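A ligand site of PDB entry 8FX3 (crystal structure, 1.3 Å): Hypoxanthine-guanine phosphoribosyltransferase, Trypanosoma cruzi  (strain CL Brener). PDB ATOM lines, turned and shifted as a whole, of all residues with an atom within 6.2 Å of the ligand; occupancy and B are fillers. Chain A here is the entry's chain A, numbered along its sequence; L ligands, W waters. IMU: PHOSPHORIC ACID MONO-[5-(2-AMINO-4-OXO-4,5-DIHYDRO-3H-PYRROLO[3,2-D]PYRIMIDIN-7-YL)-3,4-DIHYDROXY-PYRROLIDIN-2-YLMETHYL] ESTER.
The backbone NH (N) of Ser 149 sits at hydrogen-bond distance from an oxygen (O1P) of the ligand (2.9 Å).
The side-chain hydroxyl of Ser 149 is in hydrogen-bond range of an oxygen (O1P) of the ligand.
The side-chain carboxylate (OD2) of Asp 145 lies within hydrogen-bond range of an oxygen (O2') of the ligand (2.7 Å).
The backbone NH of Thr 152 is in hydrogen-bond range of an oxygen (O3P) of the ligand.
An oxygen (O3P) of the ligand lies within hydrogen-bond range of the side-chain hydroxyl of Thr 152, 2.7 Å away.
O6 of the ligand sits at hydrogen-bond distance from NZ of Lys 177, at 2.8 Å.
N of Val 199 lies within hydrogen-bond range of O6 of the ligand (2.9 Å).
N1 of the ligand is in hydrogen-bond range of O of Val 199, at 2.9 Å.
The backbone NH (N) of Asp 148 is in hydrogen-bond range of an oxygen (O2P) of the ligand (3.0 Å).
A nitrogen (N7) of the ligand lies within hydrogen-bond range of the side-chain carboxylate (OD2) of Asp 148 (3.0 Å).
The backbone NH (N) of Gly 150 is in hydrogen-bond range of an oxygen (O2P) of the ligand, at 3.0 Å.
The backbone carbonyl oxygen (O) of Glu 205 is in hydrogen-bond range of a nitrogen (N2) of the ligand (3.2 Å).
N2 of the ligand sits at hydrogen-bond distance from OE2 of Glu 205, at 3.4 Å.
The side-chain hydroxyl (OH) of Tyr 198 lies within hydrogen-bond range of a nitrogen (N2) of the ligand (3.3 Å).
N of Lys 151 is in hydrogen-bond range of OG of Ser 149.
The side-chain amino group (NZ) of Lys 177 lies within salt-bridge range of the side-chain carboxylate (OD2) of Asp 148.
The side-chain amino group of Lys 177 sits at hydrogen-bond distance from the backbone carbonyl oxygen of Lys 197, 2.9 Å away.
The backbone NH (N) of Lys 177 is in hydrogen-bond range of the backbone carbonyl oxygen (O) of Val 147 (3.1 Å).
The backbone carbonyl oxygen (O) of Glu 205 lies within hydrogen-bond range of the side-chain hydroxyl (OH) of Tyr 198, 2.7 Å away.
Merely in contact with the ligand: Phe 204 (3.6 Å), Lys 151 (3.6 Å), Lys 197 (3.7 Å), Ile 146 (3.7 Å) and Val 147 (3.99 Å).
Hydrophobic or aromatic side chains that line the ligand: Ile 146, Tyr 198, Val 199 and Phe 204.
Within 4 Å of the ligand: Asp 145, Ile 146, Val 147, Asp 148, Ser 149, Gly 150, Lys 151, Thr 152, Lys 177, Lys 197, Tyr 198, Val 199, Phe 204 and Glu 205.
Along chain A the residues within 4 Å of the ligand span positions 145 to 205.
Water W3 bridges an oxygen (O3') of the ligand (2.5 Å) and the side-chain carboxylate of Glu 144 (2.8 Å).
Water W1 lies within hydrogen-bond range of O2P of the ligand (2.7 Å) and N of Leu 153 (3.0 Å).
Water W4 lies within hydrogen-bond range of the backbone carbonyl oxygen of Ile 146 and the side-chain carboxylate of Glu 144.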
ATOM      1  N   VAL A  83     -18.941 -14.931 -17.961  1.00  0.00           N
ATOM      2  CA  VAL A  83     -17.690 -15.417 -18.605  1.00  0.00           C
ATOM      3  C   VAL A  83     -17.900 -16.847 -19.102  1.00  0.00           C
ATOM      4  O   VAL A  83     -18.018 -17.748 -18.303  1.00  0.00           O
ATOM      5  CB  VAL A  83     -16.512 -15.292 -17.613  1.00  0.00           C
ATOM      6  CG1 VAL A  83     -15.191 -15.718 -18.268  1.00  0.00           C
ATOM      7  CG2 VAL A  83     -16.393 -13.864 -17.050  1.00  0.00           C
ATOM      8  N   GLY A  86     -17.474 -21.720 -18.712  1.00  0.00           N
ATOM      9  CA  GLY A  86     -17.659 -22.301 -17.369  1.00  0.00           C
ATOM     10  C   GLY A  86     -18.782 -21.702 -16.535  1.00  0.00           C
ATOM     11  O   GLY A  86     -19.290 -22.403 -15.671  1.00  0.00           O
ATOM     12  N   VAL A 112     -12.635 -15.685 -22.584  1.00  0.00           N
ATOM     13  CA  VAL A 112     -11.166 -15.503 -22.649  1.00  0.00           C
ATOM     14  C   VAL A 112     -10.529 -16.883 -22.608  1.00  0.00           C
ATOM     15  O   VAL A 112     -11.205 -17.849 -22.300  1.00  0.00           O
ATOM     16  CB  VAL A 112     -10.625 -14.575 -21.531  1.00  0.00           C
ATOM     17  CG1 VAL A 112     -11.145 -13.132 -21.687  1.00  0.00           C
ATOM     18  CG2 VAL A 112     -10.925 -15.096 -20.127  1.00  0.00           C
ATOM     19  N   MET A 124      -2.954 -14.207 -21.654  1.00  0.00           N
ATOM     20  CA  MET A 124      -4.430 -14.150 -21.826  1.00  0.00           C
ATOM     21  C   MET A 124      -4.817 -13.536 -23.173  1.00  0.00           C
ATOM     22  O   MET A 124      -4.149 -12.613 -23.585  1.00  0.00           O
ATOM     23  CB  MET A 124      -5.065 -13.300 -20.724  1.00  0.00           C
ATOM     24  CG  MET A 124      -4.909 -13.887 -19.300  1.00  0.00           C
ATOM     25  SD  MET A 124      -5.666 -15.518 -19.148  1.00  0.00           S
ATOM     26  CE  MET A 124      -7.345 -15.175 -19.673  1.00  0.00           C
ATOM     27  N   GLU A 144     -18.391 -15.162 -12.871  1.00  0.00           N
ATOM     28  CA  GLU A 144     -17.298 -16.067 -13.269  1.00  0.00           C
ATOM     29  C   GLU A 144     -17.406 -17.367 -12.456  1.00  0.00           C
ATOM     30  O   GLU A 144     -17.965 -17.346 -11.373  1.00  0.00           O
ATOM     31  CB  GLU A 144     -15.954 -15.337 -13.063  1.00  0.00           C
ATOM     32  CG  GLU A 144     -14.685 -16.173 -13.294  1.00  0.00           C
ATOM     33  CD  GLU A 144     -14.479 -16.716 -14.707  1.00  0.00           C
ATOM     34  OE1 GLU A 144     -13.377 -16.611 -15.250  1.00  0.00           O
ATOM     35  OE2 GLU A 144     -15.417 -17.285 -15.246  1.00  0.00           O
ATOM     36  N   ASP A 145     -16.907 -18.462 -12.995  1.00  0.00           N
ATOM     37  CA  ASP A 145     -17.005 -19.794 -12.357  1.00  0.00           C
ATOM     38  C   ASP A 145     -16.091 -19.884 -11.122  1.00  0.00           C
ATOM     39  O   ASP A 145     -16.564 -20.303 -10.079  1.00  0.00           O
ATOM     40  CB  ASP A 145     -16.691 -20.905 -13.390  1.00  0.00           C
ATOM     41  CG  ASP A 145     -15.368 -20.811 -14.157  1.00  0.00           C
ATOM     42  OD1 ASP A 145     -14.610 -19.865 -13.960  1.00  0.00           O
ATOM     43  OD2 ASP A 145     -15.119 -21.691 -14.967  1.00  0.00           O
ATOM     44  N   ILE A 146     -14.823 -19.539 -11.264  1.00  0.00           N
ATOM     45  CA  ILE A 146     -13.843 -19.721 -10.156  1.00  0.00           C
ATOM     46  C   ILE A 146     -12.689 -18.731 -10.241  1.00  0.00           C
ATOM     47  O   ILE A 146     -12.307 -18.373 -11.348  1.00  0.00           O
ATOM     48  CB  ILE A 146     -13.287 -21.174 -10.152  1.00  0.00           C
ATOM     49  CG1 ILE A 146     -12.479 -21.493  -8.877  1.00  0.00           C
ATOM     50  CG2 ILE A 146     -12.477 -21.466 -11.420  1.00  0.00           C
ATOM     51  CD1 ILE A 146     -12.277 -23.002  -8.632  1.00  0.00           C
ATOM     52  N   VAL A 147     -12.185 -18.321  -9.080  1.00  0.00           N
ATOM     53  CA  VAL A 147     -10.927 -17.543  -8.995  1.00  0.00           C
ATOM     54  C   VAL A 147      -9.904 -18.545  -8.422  1.00  0.00           C
ATOM     55  O   VAL A 147     -10.185 -19.133  -7.382  1.00  0.00           O
ATOM     56  CB  VAL A 147     -11.080 -16.257  -8.169  1.00  0.00           C
ATOM     57  CG1 VAL A 147     -11.576 -16.496  -6.738  1.00  0.00           C
ATOM     58  CG2 VAL A 147      -9.766 -15.457  -8.164  1.00  0.00           C
ATOM     59  N   ASP A 148      -8.807 -18.774  -9.119  1.00  0.00           N
ATOM     60  CA  ASP A 148      -7.748 -19.726  -8.702  1.00  0.00           C
ATOM     61  C   ASP A 148      -6.480 -18.866  -8.546  1.00  0.00           C
ATOM     62  O   ASP A 148      -6.315 -18.289  -7.494  1.00  0.00           O
ATOM     63  CB  ASP A 148      -7.726 -20.907  -9.703  1.00  0.00           C
ATOM     64  CG  ASP A 148      -6.855 -22.067  -9.276  1.00  0.00           C
ATOM     65  OD1 ASP A 148      -5.988 -21.862  -8.431  1.00  0.00           O
ATOM     66  OD2 ASP A 148      -7.025 -23.171  -9.807  1.00  0.00           O
ATOM     67  N   SER A 149      -5.644 -18.724  -9.564  1.00  0.00           N
ATOM     68  CA  SER A 149      -4.452 -17.836  -9.528  1.00  0.00           C
ATOM     69  C   SER A 149      -4.887 -16.365  -9.513  1.00  0.00           C
ATOM     70  O   SER A 149      -4.137 -15.564  -8.982  1.00  0.00           O
ATOM     71  CB  SER A 149      -3.469 -18.079 -10.675  1.00  0.00           C
ATOM     72  OG  SER A 149      -3.892 -17.494 -11.895  1.00  0.00           O
ATOM     73  N   GLY A 150      -6.029 -16.039 -10.098  1.00  0.00           N
ATOM     74  CA  GLY A 150      -6.529 -14.653 -10.213  1.00  0.00           C
ATOM     75  C   GLY A 150      -6.149 -13.987 -11.543  1.00  0.00           C
ATOM     76  O   GLY A 150      -6.631 -12.904 -11.800  1.00  0.00           O
ATOM     77  N   LYS A 151      -5.329 -14.630 -12.367  1.00  0.00           N
ATOM     78  CA  LYS A 151      -4.806 -14.008 -13.614  1.00  0.00           C
ATOM     79  C   LYS A 151      -5.950 -13.772 -14.608  1.00  0.00           C
ATOM     80  O   LYS A 151      -5.986 -12.733 -15.208  1.00  0.00           O
ATOM     81  CB  LYS A 151      -3.675 -14.859 -14.213  1.00  0.00           C
ATOM     82  CG  LYS A 151      -2.389 -14.897 -13.382  1.00  0.00           C
ATOM     83  CD  LYS A 151      -1.316 -15.893 -13.944  1.00  0.00           C
ATOM     84  CE  LYS A 151      -0.747 -16.862 -12.892  1.00  0.00           C
ATOM     85  NZ  LYS A 151      -0.693 -18.287 -13.386  1.00  0.00           N
ATOM     86  N   THR A 152      -6.868 -14.725 -14.746  1.00  0.00           N
ATOM     87  CA  THR A 152      -7.975 -14.612 -15.723  1.00  0.00           C
ATOM     88  C   THR A 152      -8.827 -13.388 -15.363  1.00  0.00           C
ATOM     89  O   THR A 152      -9.082 -12.558 -16.227  1.00  0.00           O
ATOM     90  CB  THR A 152      -8.812 -15.907 -15.819  1.00  0.00           C
ATOM     91  OG1 THR A 152      -7.984 -16.978 -16.287  1.00  0.00           O
ATOM     92  CG2 THR A 152     -10.027 -15.766 -16.718  1.00  0.00           C
ATOM     93  N   LEU A 153      -9.239 -13.268 -14.110  1.00  0.00           N
ATOM     94  CA  LEU A 153     -10.135 -12.163 -13.683  1.00  0.00           C
ATOM     95  C   LEU A 153      -9.387 -10.807 -13.704  1.00  0.00           C
ATOM     96  O   LEU A 153      -9.998  -9.830 -14.026  1.00  0.00           O
ATOM     97  CB  LEU A 153     -10.734 -12.457 -12.296  1.00  0.00           C
ATOM     98  CG  LEU A 153     -12.014 -13.310 -12.299  1.00  0.00           C
ATOM     99  CD1 LEU A 153     -12.351 -13.790 -10.879  1.00  0.00           C
ATOM    100  CD2 LEU A 153     -13.205 -12.538 -12.906  1.00  0.00           C
ATOM    101  N   LYS A 177     -10.997 -20.612  -4.804  1.00  0.00           N
ATOM    102  CA  LYS A 177      -9.948 -21.582  -4.411  1.00  0.00           C
ATOM    103  C   LYS A 177      -8.887 -20.706  -3.729  1.00  0.00           C
ATOM    104  O   LYS A 177      -7.999 -20.211  -4.412  1.00  0.00           O
ATOM    105  CB  LYS A 177      -9.413 -22.363  -5.611  1.00  0.00           C
ATOM    106  CG  LYS A 177      -8.471 -23.509  -5.246  1.00  0.00           C
ATOM    107  CD  LYS A 177      -7.833 -24.193  -6.461  1.00  0.00           C
ATOM    108  CE  LYS A 177      -8.843 -24.693  -7.482  1.00  0.00           C
ATOM    109  NZ  LYS A 177      -8.170 -25.466  -8.572  1.00  0.00           N
ATOM    110  N   GLY A 180      -4.868 -21.026  -4.334  1.00  0.00           N
ATOM    111  CA  GLY A 180      -4.345 -20.901  -5.692  1.00  0.00           C
ATOM    112  C   GLY A 180      -3.843 -19.515  -6.044  1.00  0.00           C
ATOM    113  O   GLY A 180      -3.172 -19.396  -7.035  1.00  0.00           O
ATOM    114  N   VAL A 194     -13.717 -23.726  -2.231  1.00  0.00           N
ATOM    115  CA  VAL A 194     -13.363 -25.098  -2.648  1.00  0.00           C
ATOM    116  C   VAL A 194     -11.951 -25.411  -2.152  1.00  0.00           C
ATOM    117  O   VAL A 194     -11.195 -24.477  -1.937  1.00  0.00           O
ATOM    118  CB  VAL A 194     -13.481 -25.260  -4.185  1.00  0.00           C
ATOM    119  CG1 VAL A 194     -14.921 -24.981  -4.649  1.00  0.00           C
ATOM    120  CG2 VAL A 194     -12.481 -24.376  -4.959  1.00  0.00           C
ATOM    121  N   LYS A 197      -7.572 -27.891  -5.121  1.00  0.00           N
ATOM    122  CA  LYS A 197      -7.539 -29.086  -5.962  1.00  0.00           C
ATOM    123  C   LYS A 197      -8.326 -28.756  -7.233  1.00  0.00           C
ATOM    124  O   LYS A 197      -9.092 -27.837  -7.205  1.00  0.00           O
ATOM    125  CB  LYS A 197      -8.231 -30.259  -5.249  1.00  0.00           C
ATOM    126  CG  LYS A 197      -7.611 -30.747  -3.939  1.00  0.00           C
ATOM    127  CD  LYS A 197      -6.301 -31.510  -4.133  1.00  0.00           C
ATOM    128  CE  LYS A 197      -5.779 -32.165  -2.853  1.00  0.00           C
ATOM    129  NZ  LYS A 197      -4.512 -32.932  -3.099  1.00  0.00           N
ATOM    130  N   TYR A 198      -8.153 -29.548  -8.264  1.00  0.00           N
ATOM    131  CA  TYR A 198      -8.893 -29.365  -9.533  1.00  0.00           C
ATOM    132  C   TYR A 198     -10.343 -29.813  -9.317  1.00  0.00           C
ATOM    133  O   TYR A 198     -10.550 -30.969  -8.988  1.00  0.00           O
ATOM    134  CB  TYR A 198      -8.226 -30.147 -10.678  1.00  0.00           C
ATOM    135  CG  TYR A 198      -8.758 -29.758 -12.031  1.00  0.00           C
ATOM    136  CD1 TYR A 198      -9.882 -30.368 -12.575  1.00  0.00           C
ATOM    137  CD2 TYR A 198      -8.151 -28.751 -12.767  1.00  0.00           C
ATOM    138  CE1 TYR A 198     -10.369 -30.002 -13.823  1.00  0.00           C
ATOM    139  CE2 TYR A 198      -8.633 -28.377 -14.010  1.00  0.00           C
ATOM    140  CZ  TYR A 198      -9.736 -29.007 -14.547  1.00  0.00           C
ATOM    141  OH  TYR A 198     -10.167 -28.619 -15.779  1.00  0.00           O
ATOM    142  N   VAL A 199     -11.293 -28.909  -9.502  1.00  0.00           N
ATOM    143  CA  VAL A 199     -12.742 -29.218  -9.286  1.00  0.00           C
ATOM    144  C   VAL A 199     -13.446 -29.523 -10.616  1.00  0.00           C
ATOM    145  O   VAL A 199     -13.036 -29.017 -11.643  1.00  0.00           O
ATOM    146  CB  VAL A 199     -13.477 -28.117  -8.485  1.00  0.00           C
ATOM    147  CG1 VAL A 199     -12.969 -28.069  -7.033  1.00  0.00           C
ATOM    148  CG2 VAL A 199     -13.391 -26.730  -9.148  1.00  0.00           C
ATOM    149  N   ILE A 200     -14.489 -30.337 -10.561  1.00  0.00           N
ATOM    150  CA  ILE A 200     -15.309 -30.737 -11.738  1.00  0.00           C
ATOM    151  C   ILE A 200     -16.774 -30.700 -11.303  1.00  0.00           C
ATOM    152  O   ILE A 200     -17.036 -30.788 -10.116  1.00  0.00           O
ATOM    153  CB  ILE A 200     -14.912 -32.120 -12.292  1.00  0.00           C
ATOM    154  CG1 ILE A 200     -14.995 -33.208 -11.196  1.00  0.00           C
ATOM    155  CG2 ILE A 200     -13.526 -32.075 -12.953  1.00  0.00           C
ATOM    156  CD1 ILE A 200     -15.119 -34.638 -11.751  1.00  0.00           C
ATOM    157  N   GLY A 203     -20.642 -26.974 -14.237  1.00  0.00           N
ATOM    158  CA  GLY A 203     -19.912 -26.024 -15.102  1.00  0.00           C
ATOM    159  C   GLY A 203     -18.442 -26.329 -15.200  1.00  0.00           C
ATOM    160  O   GLY A 203     -17.864 -25.951 -16.207  1.00  0.00           O
ATOM    161  N   PHE A 204     -17.858 -26.975 -14.197  1.00  0.00           N
ATOM    162  CA  PHE A 204     -16.406 -27.267 -14.144  1.00  0.00           C
ATOM    163  C   PHE A 204     -16.137 -28.519 -14.985  1.00  0.00           C
ATOM    164  O   PHE A 204     -16.786 -29.527 -14.761  1.00  0.00           O
ATOM    165  CB  PHE A 204     -15.875 -27.400 -12.716  1.00  0.00           C
ATOM    166  CG  PHE A 204     -15.971 -26.110 -11.928  1.00  0.00           C
ATOM    167  CD1 PHE A 204     -15.258 -24.992 -12.320  1.00  0.00           C
ATOM    168  CD2 PHE A 204     -16.802 -26.015 -10.814  1.00  0.00           C
ATOM    169  CE1 PHE A 204     -15.347 -23.810 -11.602  1.00  0.00           C
ATOM    170  CE2 PHE A 204     -16.887 -24.830 -10.104  1.00  0.00           C
ATOM    171  CZ  PHE A 204     -16.172 -23.726 -10.499  1.00  0.00           C
ATOM    172  N   GLU A 205     -15.166 -28.432 -15.880  1.00  0.00           N
ATOM    173  CA  GLU A 205     -14.948 -29.502 -16.884  1.00  0.00           C
ATOM    174  C   GLU A 205     -13.565 -30.126 -16.950  1.00  0.00           C
ATOM    175  O   GLU A 205     -12.669 -29.592 -16.326  1.00  0.00           O
ATOM    176  CB  GLU A 205     -15.202 -28.860 -18.274  1.00  0.00           C
ATOM    177  CG  GLU A 205     -14.012 -28.171 -18.976  1.00  0.00           C
ATOM    178  CD  GLU A 205     -13.438 -26.886 -18.385  1.00  0.00           C
ATOM    179  OE1 GLU A 205     -12.621 -26.245 -19.085  1.00  0.00           O
ATOM    180  OE2 GLU A 205     -13.804 -26.497 -17.267  1.00  0.00           O
ATOM    181  N   VAL A 206     -13.464 -31.265 -17.622  1.00  0.00           N
ATOM    182  CA  VAL A 206     -12.200 -31.867 -18.104  1.00  0.00           C
ATOM    183  C   VAL A 206     -12.466 -32.048 -19.615  1.00  0.00           C
ATOM    184  O   VAL A 206     -13.260 -32.906 -19.936  1.00  0.00           O
ATOM    185  CB  VAL A 206     -11.804 -33.183 -17.420  1.00  0.00           C
ATOM    186  CG1 VAL A 206     -10.619 -33.857 -18.133  1.00  0.00           C
ATOM    187  CG2 VAL A 206     -11.492 -32.973 -15.932  1.00  0.00           C
HETATM  188  P   IMU L   1      -7.099 -18.480 -12.833  1.00  0.00           P
HETATM  189  C2  IMU L   1     -11.742 -26.345 -13.461  1.00  0.00           C
HETATM  190  O1P IMU L   1      -5.897 -19.279 -12.350  1.00  0.00           O
HETATM  191  O2P IMU L   1      -7.862 -17.800 -11.767  1.00  0.00           O
HETATM  192  O3P IMU L   1      -6.662 -17.546 -13.963  1.00  0.00           O
HETATM  193  O5' IMU L   1      -8.122 -19.654 -13.473  1.00  0.00           O
HETATM  194  C5' IMU L   1      -9.455 -19.485 -13.789  1.00  0.00           C
HETATM  195  C4' IMU L   1      -9.733 -19.992 -15.176  1.00  0.00           C
HETATM  196  N4' IMU L   1      -9.163 -21.495 -15.327  1.00  0.00           N
HETATM  197  C3' IMU L   1     -11.017 -20.074 -15.488  1.00  0.00           C
HETATM  198  O3' IMU L   1     -11.224 -20.051 -17.002  1.00  0.00           O
HETATM  199  C2' IMU L   1     -11.422 -21.457 -14.942  1.00  0.00           C
HETATM  200  O2' IMU L   1     -12.492 -21.911 -15.667  1.00  0.00           O
HETATM  201  C1' IMU L   1     -10.138 -22.340 -15.084  1.00  0.00           C
HETATM  202  C9  IMU L   1      -9.944 -23.131 -13.708  1.00  0.00           C
HETATM  203  C8  IMU L   1      -9.184 -22.742 -12.595  1.00  0.00           C
HETATM  204  N7  IMU L   1      -9.293 -23.681 -11.659  1.00  0.00           N
HETATM  205  C5  IMU L   1     -10.096 -24.692 -12.087  1.00  0.00           C
HETATM  206  C6  IMU L   1     -10.545 -25.939 -11.399  1.00  0.00           C
HETATM  207  O6  IMU L   1     -10.236 -26.284 -10.324  1.00  0.00           O
HETATM  208  N1  IMU L   1     -11.357 -26.719 -12.167  1.00  0.00           N
HETATM  209  N2  IMU L   1     -12.629 -27.231 -14.152  1.00  0.00           N
HETATM  210  N3  IMU L   1     -11.370 -25.178 -14.125  1.00  0.00           N
HETATM  211  C4  IMU L   1     -10.498 -24.347 -13.364  1.00  0.00           C
HETATM  212  O   HOH W   1      -9.219 -15.525 -12.151  1.00  0.00           O
HETATM  213  O   HOH W   2      -4.617 -18.480 -15.502  1.00  0.00           O
HETATM  214  O   HOH W   3     -12.650 -18.104 -17.492  1.00  0.00           O
HETATM  215  O   HOH W   4     -11.369 -16.757 -13.330  1.00  0.00           O
HETATM  216  O   HOH W   5      -5.160 -21.736 -12.741  1.00  0.00           O
